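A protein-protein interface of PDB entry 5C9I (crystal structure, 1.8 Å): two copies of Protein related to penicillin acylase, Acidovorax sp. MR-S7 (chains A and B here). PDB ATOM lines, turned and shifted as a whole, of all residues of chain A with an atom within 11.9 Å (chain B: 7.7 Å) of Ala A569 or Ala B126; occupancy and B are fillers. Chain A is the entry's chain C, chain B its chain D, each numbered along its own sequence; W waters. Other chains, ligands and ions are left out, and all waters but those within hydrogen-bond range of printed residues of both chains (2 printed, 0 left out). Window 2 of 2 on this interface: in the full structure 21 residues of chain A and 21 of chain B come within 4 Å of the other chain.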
ATOM      1  N   ILE A 557     -15.758   2.945  11.361  1.00  0.00           N
ATOM      2  CA  ILE A 557     -15.680   3.783  12.575  1.00  0.00           C
ATOM      3  C   ILE A 557     -16.385   5.127  12.507  1.00  0.00           C
ATOM      4  O   ILE A 557     -16.516   5.767  13.532  1.00  0.00           O
ATOM      5  CB  ILE A 557     -14.203   3.977  12.990  1.00  0.00           C
ATOM      6  CG1 ILE A 557     -13.483   4.885  11.980  1.00  0.00           C
ATOM      7  CG2 ILE A 557     -13.549   2.595  13.199  1.00  0.00           C
ATOM      8  CD1 ILE A 557     -12.016   5.179  12.312  1.00  0.00           C
ATOM      9  N   PRO A 560     -21.551   6.211  14.327  1.00  0.00           N
ATOM     10  CA  PRO A 560     -21.512   7.654  14.456  1.00  0.00           C
ATOM     11  C   PRO A 560     -20.059   8.180  14.433  1.00  0.00           C
ATOM     12  O   PRO A 560     -19.097   7.388  14.603  1.00  0.00           O
ATOM     13  CB  PRO A 560     -22.139   7.896  15.855  1.00  0.00           C
ATOM     14  CG  PRO A 560     -21.744   6.697  16.649  1.00  0.00           C
ATOM     15  CD  PRO A 560     -21.756   5.537  15.633  1.00  0.00           C
ATOM     16  N   ALA A 561     -19.927   9.483  14.160  1.00  0.00           N
ATOM     17  CA  ALA A 561     -18.672  10.148  14.180  1.00  0.00           C
ATOM     18  C   ALA A 561     -18.424  10.784  15.533  1.00  0.00           C
ATOM     19  O   ALA A 561     -17.383  11.401  15.709  1.00  0.00           O
ATOM     20  CB  ALA A 561     -18.632  11.215  13.073  1.00  0.00           C
ATOM     21  N   GLN A 562     -19.380  10.708  16.449  1.00  0.00           N
ATOM     22  CA  GLN A 562     -19.072  11.088  17.862  1.00  0.00           C
ATOM     23  C   GLN A 562     -18.698   9.844  18.619  1.00  0.00           C
ATOM     24  O   GLN A 562     -19.458   8.875  18.641  1.00  0.00           O
ATOM     25  CB  GLN A 562     -20.236  11.798  18.539  1.00  0.00           C
ATOM     26  CG  GLN A 562     -20.825  12.844  17.642  1.00  0.00           C
ATOM     27  CD  GLN A 562     -19.792  13.905  17.323  1.00  0.00           C
ATOM     28  OE1 GLN A 562     -19.056  14.398  18.218  1.00  0.00           O
ATOM     29  NE2 GLN A 562     -19.694  14.253  16.027  1.00  0.00           N
ATOM     30  N   TRP A 563     -17.516   9.848  19.239  1.00  0.00           N
ATOM     31  CA  TRP A 563     -16.979   8.632  19.842  1.00  0.00           C
ATOM     32  C   TRP A 563     -16.697   8.806  21.306  1.00  0.00           C
ATOM     33  O   TRP A 563     -16.584   9.945  21.775  1.00  0.00           O
ATOM     34  CB  TRP A 563     -15.656   8.307  19.178  1.00  0.00           C
ATOM     35  CG  TRP A 563     -15.666   8.106  17.657  1.00  0.00           C
ATOM     36  CD1 TRP A 563     -16.726   7.757  16.803  1.00  0.00           C
ATOM     37  CD2 TRP A 563     -14.494   8.154  16.804  1.00  0.00           C
ATOM     38  NE1 TRP A 563     -16.292   7.644  15.491  1.00  0.00           N
ATOM     39  CE2 TRP A 563     -14.943   7.844  15.443  1.00  0.00           C
ATOM     40  CE3 TRP A 563     -13.169   8.413  17.027  1.00  0.00           C
ATOM     41  CZ2 TRP A 563     -14.069   7.808  14.389  1.00  0.00           C
ATOM     42  CZ3 TRP A 563     -12.281   8.360  15.949  1.00  0.00           C
ATOM     43  CH2 TRP A 563     -12.729   8.074  14.663  1.00  0.00           C
ATOM     44  N   THR A 564     -16.522   7.681  22.010  1.00  0.00           N
ATOM     45  CA  THR A 564     -15.776   7.641  23.292  1.00  0.00           C
ATOM     46  C   THR A 564     -14.462   6.847  23.083  1.00  0.00           C
ATOM     47  O   THR A 564     -14.462   5.697  22.625  1.00  0.00           O
ATOM     48  CB  THR A 564     -16.636   7.048  24.424  1.00  0.00           C
ATOM     49  OG1 THR A 564     -17.926   7.690  24.411  1.00  0.00           O
ATOM     50  CG2 THR A 564     -15.965   7.263  25.792  1.00  0.00           C
ATOM     51  N   VAL A 565     -13.323   7.476  23.359  1.00  0.00           N
ATOM     52  CA  VAL A 565     -12.018   6.817  23.154  1.00  0.00           C
ATOM     53  C   VAL A 565     -11.235   6.989  24.438  1.00  0.00           C
ATOM     54  O   VAL A 565     -11.052   8.137  24.852  1.00  0.00           O
ATOM     55  CB  VAL A 565     -11.210   7.515  21.968  1.00  0.00           C
ATOM     56  CG1 VAL A 565      -9.764   6.994  21.825  1.00  0.00           C
ATOM     57  CG2 VAL A 565     -11.939   7.418  20.660  1.00  0.00           C
ATOM     58  N   ASN A 566     -10.796   5.901  25.093  1.00  0.00           N
ATOM     59  CA  ASN A 566     -10.089   6.053  26.385  1.00  0.00           C
ATOM     60  C   ASN A 566     -10.879   6.906  27.362  1.00  0.00           C
ATOM     61  O   ASN A 566     -10.311   7.753  28.080  1.00  0.00           O
ATOM     62  CB  ASN A 566      -8.717   6.691  26.150  1.00  0.00           C
ATOM     63  CG  ASN A 566      -7.897   5.883  25.184  1.00  0.00           C
ATOM     64  OD1 ASN A 566      -7.814   4.687  25.365  1.00  0.00           O
ATOM     65  ND2 ASN A 566      -7.306   6.503  24.185  1.00  0.00           N
ATOM     66  N   GLY A 567     -12.197   6.701  27.356  1.00  0.00           N
ATOM     67  CA  GLY A 567     -13.103   7.385  28.269  1.00  0.00           C
ATOM     68  C   GLY A 567     -13.321   8.869  27.971  1.00  0.00           C
ATOM     69  O   GLY A 567     -13.984   9.549  28.775  1.00  0.00           O
ATOM     70  N   ALA A 568     -12.895   9.322  26.798  1.00  0.00           N
ATOM     71  CA  ALA A 568     -13.047  10.735  26.362  1.00  0.00           C
ATOM     72  C   ALA A 568     -13.946  10.863  25.190  1.00  0.00           C
ATOM     73  O   ALA A 568     -13.839  10.059  24.206  1.00  0.00           O
ATOM     74  CB  ALA A 568     -11.687  11.341  25.972  1.00  0.00           C
ATOM     75  N   ALA A 569     -14.795  11.890  25.229  1.00  0.00           N
ATOM     76  CA  ALA A 569     -15.618  12.242  24.071  1.00  0.00           C
ATOM     77  C   ALA A 569     -14.740  12.780  22.939  1.00  0.00           C
ATOM     78  O   ALA A 569     -14.044  13.785  23.102  1.00  0.00           O
ATOM     79  CB  ALA A 569     -16.693  13.255  24.453  1.00  0.00           C
ATOM     80  N   VAL A 570     -14.804  12.123  21.797  1.00  0.00           N
ATOM     81  CA  VAL A 570     -14.027  12.519  20.621  1.00  0.00           C
ATOM     82  C   VAL A 570     -15.028  12.827  19.460  1.00  0.00           C
ATOM     83  O   VAL A 570     -15.816  11.959  19.047  1.00  0.00           O
ATOM     84  CB  VAL A 570     -12.995  11.471  20.193  1.00  0.00           C
ATOM     85  CG1 VAL A 570     -12.391  11.847  18.817  1.00  0.00           C
ATOM     86  CG2 VAL A 570     -11.889  11.361  21.245  1.00  0.00           C
ATOM     87  N   ASP A 571     -14.952  14.042  18.950  1.00  0.00           N
ATOM     88  CA  ASP A 571     -15.722  14.460  17.786  1.00  0.00           C
ATOM     89  C   ASP A 571     -14.910  14.268  16.523  1.00  0.00           C
ATOM     90  O   ASP A 571     -14.087  15.094  16.170  1.00  0.00           O
ATOM     91  CB  ASP A 571     -16.109  15.919  17.934  1.00  0.00           C
ATOM     92  CG  ASP A 571     -16.977  16.407  16.823  1.00  0.00           C
ATOM     93  OD1 ASP A 571     -17.173  15.752  15.773  1.00  0.00           O
ATOM     94  OD2 ASP A 571     -17.530  17.477  17.039  1.00  0.00           O
ATOM     95  N   ALA A 572     -15.158  13.133  15.862  1.00  0.00           N
ATOM     96  CA  ALA A 572     -14.414  12.795  14.641  1.00  0.00           C
ATOM     97  C   ALA A 572     -15.158  13.207  13.369  1.00  0.00           C
ATOM     98  O   ALA A 572     -14.759  12.797  12.279  1.00  0.00           O
ATOM     99  CB  ALA A 572     -14.166  11.280  14.582  1.00  0.00           C
ATOM    100  N   ALA A 573     -16.230  14.007  13.475  1.00  0.00           N
ATOM    101  CA  ALA A 573     -17.048  14.313  12.256  1.00  0.00           C
ATOM    102  C   ALA A 573     -16.201  15.008  11.183  1.00  0.00           C
ATOM    103  O   ALA A 573     -16.310  14.672  10.003  1.00  0.00           O
ATOM    104  CB  ALA A 573     -18.225  15.215  12.608  1.00  0.00           C
ATOM    105  N   GLN A 574     -15.412  16.019  11.575  1.00  0.00           N
ATOM    106  CA  GLN A 574     -14.564  16.663  10.566  1.00  0.00           C
ATOM    107  C   GLN A 574     -13.528  15.706   9.967  1.00  0.00           C
ATOM    108  O   GLN A 574     -13.341  15.712   8.726  1.00  0.00           O
ATOM    109  CB  GLN A 574     -13.883  17.958  11.052  1.00  0.00           C
ATOM    110  CG  GLN A 574     -13.080  18.620   9.921  1.00  0.00           C
ATOM    111  CD  GLN A 574     -12.221  19.805  10.387  1.00  0.00           C
ATOM    112  OE1 GLN A 574     -11.758  19.855  11.518  1.00  0.00           O
ATOM    113  NE2 GLN A 574     -11.954  20.728   9.478  1.00  0.00           N
ATOM    114  N   ARG A 634     -10.239   3.601  16.076  1.00  0.00           N
ATOM    115  CA  ARG A 634     -10.680   4.882  16.635  1.00  0.00           C
ATOM    116  C   ARG A 634      -9.557   5.490  17.531  1.00  0.00           C
ATOM    117  O   ARG A 634      -9.343   6.692  17.536  1.00  0.00           O
ATOM    118  CB  ARG A 634     -11.998   4.757  17.448  1.00  0.00           C
ATOM    119  CG  ARG A 634     -13.256   4.677  16.611  1.00  0.00           C
ATOM    120  CD  ARG A 634     -14.534   4.653  17.483  1.00  0.00           C
ATOM    121  NE  ARG A 634     -14.733   3.339  18.065  1.00  0.00           N
ATOM    122  CZ  ARG A 634     -15.460   2.367  17.508  1.00  0.00           C
ATOM    123  NH1 ARG A 634     -15.514   1.178  18.084  1.00  0.00           N
ATOM    124  NH2 ARG A 634     -16.116   2.569  16.400  1.00  0.00           N
ATOM    125  N   GLN A 635      -8.822   4.635  18.256  1.00  0.00           N
ATOM    126  CA  GLN A 635      -7.680   5.141  19.067  1.00  0.00           C
ATOM    127  C   GLN A 635      -6.628   5.764  18.202  1.00  0.00           C
ATOM    128  O   GLN A 635      -6.049   6.836  18.542  1.00  0.00           O
ATOM    129  CB  GLN A 635      -7.064   4.031  19.953  1.00  0.00           C
ATOM    130  CG  GLN A 635      -8.000   3.665  21.067  1.00  0.00           C
ATOM    131  CD  GLN A 635      -7.604   2.408  21.817  1.00  0.00           C
ATOM    132  OE1 GLN A 635      -7.124   1.405  21.228  1.00  0.00           O
ATOM    133  NE2 GLN A 635      -7.826   2.433  23.112  1.00  0.00           N
ATOM    134  N   MET A 637      -7.010   6.915  15.124  1.00  0.00           N
ATOM    135  CA  MET A 637      -7.540   8.130  14.495  1.00  0.00           C
ATOM    136  C   MET A 637      -7.567   9.287  15.473  1.00  0.00           C
ATOM    137  O   MET A 637      -7.217  10.415  15.096  1.00  0.00           O
ATOM    138  CB  MET A 637      -8.969   7.854  13.893  1.00  0.00           C
ATOM    139  CG  MET A 637      -9.452   9.025  13.041  1.00  0.00           C
ATOM    140  SD  MET A 637      -8.421   9.230  11.557  1.00  0.00           S
ATOM    141  CE  MET A 637      -9.030   7.847  10.563  1.00  0.00           C
ATOM    142  N   ALA A 638      -7.958   9.008  16.717  1.00  0.00           N
ATOM    143  CA  ALA A 638      -8.018  10.069  17.683  1.00  0.00           C
ATOM    144  C   ALA A 638      -6.586  10.623  17.923  1.00  0.00           C
ATOM    145  O   ALA A 638      -6.376  11.854  18.014  1.00  0.00           O
ATOM    146  CB  ALA A 638      -8.677   9.584  18.971  1.00  0.00           C
ATOM    147  N   THR A 639      -5.608   9.717  18.023  1.00  0.00           N
ATOM    148  CA  THR A 639      -4.205  10.192  18.094  1.00  0.00           C
ATOM    149  C   THR A 639      -3.789  11.047  16.855  1.00  0.00           C
ATOM    150  O   THR A 639      -3.158  12.114  16.995  1.00  0.00           O
ATOM    151  CB  THR A 639      -3.186   9.046  18.369  1.00  0.00           C
ATOM    152  OG1 THR A 639      -3.567   8.380  19.579  1.00  0.00           O
ATOM    153  CG2 THR A 639      -1.765   9.657  18.585  1.00  0.00           C
ATOM    154  N   ILE A 641      -5.702  12.814  14.771  1.00  0.00           N
ATOM    155  CA  ILE A 641      -6.372  14.129  14.793  1.00  0.00           C
ATOM    156  C   ILE A 641      -5.587  15.039  15.779  1.00  0.00           C
ATOM    157  O   ILE A 641      -5.321  16.205  15.491  1.00  0.00           O
ATOM    158  CB  ILE A 641      -7.836  13.921  15.289  1.00  0.00           C
ATOM    159  CG1 ILE A 641      -8.631  13.178  14.184  1.00  0.00           C
ATOM    160  CG2 ILE A 641      -8.489  15.219  15.742  1.00  0.00           C
ATOM    161  CD1 ILE A 641     -10.015  12.774  14.732  1.00  0.00           C
ATOM    162  N   ALA A 642      -5.209  14.498  16.932  1.00  0.00           N
ATOM    163  CA  ALA A 642      -4.475  15.272  17.957  1.00  0.00           C
ATOM    164  C   ALA A 642      -3.088  15.749  17.433  1.00  0.00           C
ATOM    165  O   ALA A 642      -2.702  16.891  17.640  1.00  0.00           O
ATOM    166  CB  ALA A 642      -4.343  14.504  19.306  1.00  0.00           C
ATOM    167  N   TYR B 120     -10.246  18.136  36.943  1.00  0.00           N
ATOM    168  CA  TYR B 120      -9.926  18.643  35.580  1.00  0.00           C
ATOM    169  C   TYR B 120      -9.838  17.499  34.565  1.00  0.00           C
ATOM    170  O   TYR B 120     -10.368  17.625  33.466  1.00  0.00           O
ATOM    171  CB  TYR B 120      -8.592  19.472  35.530  1.00  0.00           C
ATOM    172  CG  TYR B 120      -8.588  20.176  34.216  1.00  0.00           C
ATOM    173  CD1 TYR B 120      -9.508  21.203  33.986  1.00  0.00           C
ATOM    174  CD2 TYR B 120      -7.853  19.692  33.139  1.00  0.00           C
ATOM    175  CE1 TYR B 120      -9.665  21.763  32.712  1.00  0.00           C
ATOM    176  CE2 TYR B 120      -7.962  20.243  31.887  1.00  0.00           C
ATOM    177  CZ  TYR B 120      -8.876  21.283  31.670  1.00  0.00           C
ATOM    178  OH  TYR B 120      -8.971  21.831  30.400  1.00  0.00           O
ATOM    179  N   VAL B 121      -9.164  16.377  34.905  1.00  0.00           N
ATOM    180  CA  VAL B 121      -9.170  15.200  34.001  1.00  0.00           C
ATOM    181  C   VAL B 121     -10.622  14.818  33.564  1.00  0.00           C
ATOM    182  O   VAL B 121     -10.871  14.580  32.363  1.00  0.00           O
ATOM    183  CB  VAL B 121      -8.405  13.977  34.586  1.00  0.00           C
ATOM    184  CG1 VAL B 121      -8.627  12.756  33.725  1.00  0.00           C
ATOM    185  CG2 VAL B 121      -6.900  14.312  34.703  1.00  0.00           C
ATOM    186  N   ARG B 122     -11.563  14.741  34.513  1.00  0.00           N
ATOM    187  CA  ARG B 122     -12.961  14.455  34.158  1.00  0.00           C
ATOM    188  C   ARG B 122     -13.492  15.485  33.194  1.00  0.00           C
ATOM    189  O   ARG B 122     -14.177  15.113  32.225  1.00  0.00           O
ATOM    190  CB  ARG B 122     -13.911  14.342  35.357  1.00  0.00           C
ATOM    191  CG  ARG B 122     -13.547  13.164  36.263  1.00  0.00           C
ATOM    192  CD  ARG B 122     -14.683  12.916  37.272  1.00  0.00           C
ATOM    193  NE  ARG B 122     -14.890  14.097  38.143  1.00  0.00           N
ATOM    194  CZ  ARG B 122     -14.160  14.346  39.259  1.00  0.00           C
ATOM    195  NH1 ARG B 122     -13.129  13.520  39.571  1.00  0.00           N
ATOM    196  NH2 ARG B 122     -14.424  15.426  40.018  1.00  0.00           N
ATOM    197  N   GLU B 123     -13.145  16.750  33.413  1.00  0.00           N
ATOM    198  CA  GLU B 123     -13.726  17.778  32.546  1.00  0.00           C
ATOM    199  C   GLU B 123     -13.082  17.676  31.142  1.00  0.00           C
ATOM    200  O   GLU B 123     -13.800  17.724  30.121  1.00  0.00           O
ATOM    201  CB  GLU B 123     -13.498  19.158  33.136  1.00  0.00           C
ATOM    202  CG  GLU B 123     -14.449  19.405  34.322  1.00  0.00           C
ATOM    203  CD  GLU B 123     -14.101  20.726  35.021  1.00  0.00           C
ATOM    204  OE1 GLU B 123     -13.221  21.490  34.470  1.00  0.00           O
ATOM    205  OE2 GLU B 123     -14.680  20.928  36.119  1.00  0.00           O
ATOM    206  N   ALA B 124     -11.770  17.471  31.089  1.00  0.00           N
ATOM    207  CA  ALA B 124     -11.076  17.329  29.771  1.00  0.00           C
ATOM    208  C   ALA B 124     -11.645  16.124  29.003  1.00  0.00           C
ATOM    209  O   ALA B 124     -11.848  16.197  27.793  1.00  0.00           O
ATOM    210  CB  ALA B 124      -9.546  17.187  29.978  1.00  0.00           C
ATOM    211  N   LYS B 125     -11.920  15.005  29.688  1.00  0.00           N
ATOM    212  CA  LYS B 125     -12.422  13.831  28.969  1.00  0.00           C
ATOM    213  C   LYS B 125     -13.829  14.119  28.453  1.00  0.00           C
ATOM    214  O   LYS B 125     -14.213  13.675  27.331  1.00  0.00           O
ATOM    215  CB  LYS B 125     -12.410  12.580  29.890  1.00  0.00           C
ATOM    216  CG  LYS B 125     -11.025  12.037  30.163  1.00  0.00           C
ATOM    217  CD  LYS B 125     -11.151  10.766  30.969  1.00  0.00           C
ATOM    218  CE  LYS B 125      -9.790  10.154  31.140  1.00  0.00           C
ATOM    219  NZ  LYS B 125      -9.414   9.334  29.942  1.00  0.00           N
ATOM    220  N   ALA B 126     -14.614  14.886  29.252  1.00  0.00           N
ATOM    221  CA  ALA B 126     -16.060  15.088  28.884  1.00  0.00           C
ATOM    222  C   ALA B 126     -16.257  15.877  27.579  1.00  0.00           C
ATOM    223  O   ALA B 126     -17.249  15.665  26.893  1.00  0.00           O
ATOM    224  CB  ALA B 126     -16.850  15.757  30.021  1.00  0.00           C
ATOM    225  N   GLY B 127     -15.306  16.719  27.211  1.00  0.00           N
ATOM    226  CA  GLY B 127     -15.454  17.525  25.977  1.00  0.00           C
ATOM    227  C   GLY B 127     -14.455  18.676  25.948  1.00  0.00           C
ATOM    228  O   GLY B 127     -13.462  18.692  26.727  1.00  0.00           O
ATOM    229  N   GLY B 128     -14.715  19.665  25.091  1.00  0.00           N
ATOM    230  CA  GLY B 128     -13.878  20.863  25.068  1.00  0.00           C
ATOM    231  C   GLY B 128     -12.805  20.730  24.011  1.00  0.00           C
ATOM    232  O   GLY B 128     -12.577  19.634  23.439  1.00  0.00           O
ATOM    233  N   ARG B 135      -5.951  15.067  25.209  1.00  0.00           N
ATOM    234  CA  ARG B 135      -7.159  14.801  26.047  1.00  0.00           C
ATOM    235  C   ARG B 135      -7.796  13.404  25.797  1.00  0.00           C
ATOM    236  O   ARG B 135      -8.432  12.868  26.722  1.00  0.00           O
ATOM    237  CB  ARG B 135      -8.180  15.941  25.955  1.00  0.00           C
ATOM    238  CG  ARG B 135      -8.673  16.202  24.515  1.00  0.00           C
ATOM    239  CD  ARG B 135      -9.855  17.205  24.468  1.00  0.00           C
ATOM    240  NE  ARG B 135     -11.030  16.615  25.138  1.00  0.00           N
ATOM    241  CZ  ARG B 135     -11.881  15.788  24.516  1.00  0.00           C
ATOM    242  NH1 ARG B 135     -11.707  15.513  23.190  1.00  0.00           N
ATOM    243  NH2 ARG B 135     -12.900  15.219  25.187  1.00  0.00           N
ATOM    244  N   SER B 136      -7.582  12.784  24.622  1.00  0.00           N
ATOM    245  CA  SER B 136      -8.248  11.533  24.337  1.00  0.00           C
ATOM    246  C   SER B 136      -7.275  10.354  24.469  1.00  0.00           C
ATOM    247  O   SER B 136      -7.639   9.203  24.169  1.00  0.00           O
ATOM    248  CB  SER B 136      -8.969  11.573  22.969  1.00  0.00           C
ATOM    249  OG  SER B 136      -8.017  11.816  21.937  1.00  0.00           O
HETATM  250  O   HOH W   1     -12.906  15.866  20.034  1.00  0.00           O
HETATM  251  O   HOH W   2      -8.125  13.395  19.563  1.00  0.00           O
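The backbone carbonyl oxygen (O) of Lys B125 sits at hydrogen-bond distance from the backbone NH (N) of Ala A569, 2.8 Å away. The backbone carbonyl oxygen (O) of Asn A566 sits at hydrogen-bond distance from the side-chain amino group (NZ) of Lys B125. The guanidinium group of Arg B135 sits at hydrogen-bond distance from the backbone carbonyl oxygen of Ala A569 (2.8 Å). ND2 of Asn A566 lies within hydrogen-bond range of O of Ser B136 (2.7 Å).
The guanidinium group (NE) of Arg B135 is in hydrogen-bond range of the backbone carbonyl oxygen (O) of Ala B124 (2.8 Å). The side-chain amide nitrogen (NE2) of Gln A635 lies within hydrogen-bond range of the side-chain amide oxygen (OD1) of Asn A566 (3.2 Å). The backbone carbonyl oxygen (O) of Lys B125 is in hydrogen-bond range of the guanidinium group (NH2) of Arg B135, 3.0 Å away. The backbone NH (N) of Trp A563 sits at hydrogen-bond distance from the backbone carbonyl oxygen (O) of Val A570 (2.7 Å).
Ser B136 touches Val A565. Gly A567 touches Lys B125 (O to CB, 3.6 Å). O of Lys B125 touches CA of Ala A568, 3.3 Å away. Ala A568 touches Arg B135 (CB to O, 3.7 Å). Ala A568 touches Ser B136 (CB to CA, 3.8 Å). Ala B126 touches Ala A569 (O to CB, 3.5 Å). Val A570 touches Ser B136. Ala A638 touches Ser B136 (CB to OG, 3.8 Å).
Of the printed residues of chain B, Val A565 touches Ser B136 (3.6 Å). Of the printed residues of chain B, Asn A566 touches Lys B125 and Ser B136. Of the printed residues of chain B, Gly A567 touches Lys B125 (3.6 Å). Ala A568 touches just these residues of chain B: Lys B125 (3.3 Å), Arg B135 (3.7 Å) and Ser B136 (3.8 Å). Of the printed residues of chain B, Ala A638 touches Ser B136. Of the printed residues of chain A, Lys B125 touches Asn A566, Gly A567, Ala A568 and Ala A569. Ala B126 touches just one residue of chain A: Ala A569. No residue of chain A comes within 4 Å of Gly B127. No residue of chain A comes within 4 Å of Gly B128. Printed residues of chain A within 4 Å of Arg B135: Ala A568 and Ala A569. Ser B136 touches just these residues of chain A: Val A565 (3.6 Å), Asn A566 (2.7 Å), Ala A568 (3.8 Å), Val A570 (3.4 Å) and Ala A638 (3.8 Å). The nearest printed residue of chain B that does not touch Gly A567 is Ala B126 (5.4 Å).
Hydrophobic or aromatic side chains of chain A within 4 Å of the printed part of chain B: Val A565, Ala A568, Ala A569, Val A570 and Ala A638. Of the 11 printed residues of chain B, 4 touch a printed residue of chain A. Along chain B the printed residues that touch a printed residue of chain A span positions 125 to 136.
No position is printed for both chains. Of the 12 pairs that touch across the chains among the printed residues, none has its exchanged pair printed and touching as well.
Water W2 bridges the backbone carbonyl oxygen (O) of Ala A638 (2.8 Å) and the side-chain hydroxyl (OG) of Ser B136 (2.9 Å). Water W1 lies within hydrogen-bond range of the backbone NH (N) of Asp A571 (2.9 Å) and the guanidinium group (NH1) of Arg B135 (3.4 Å).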
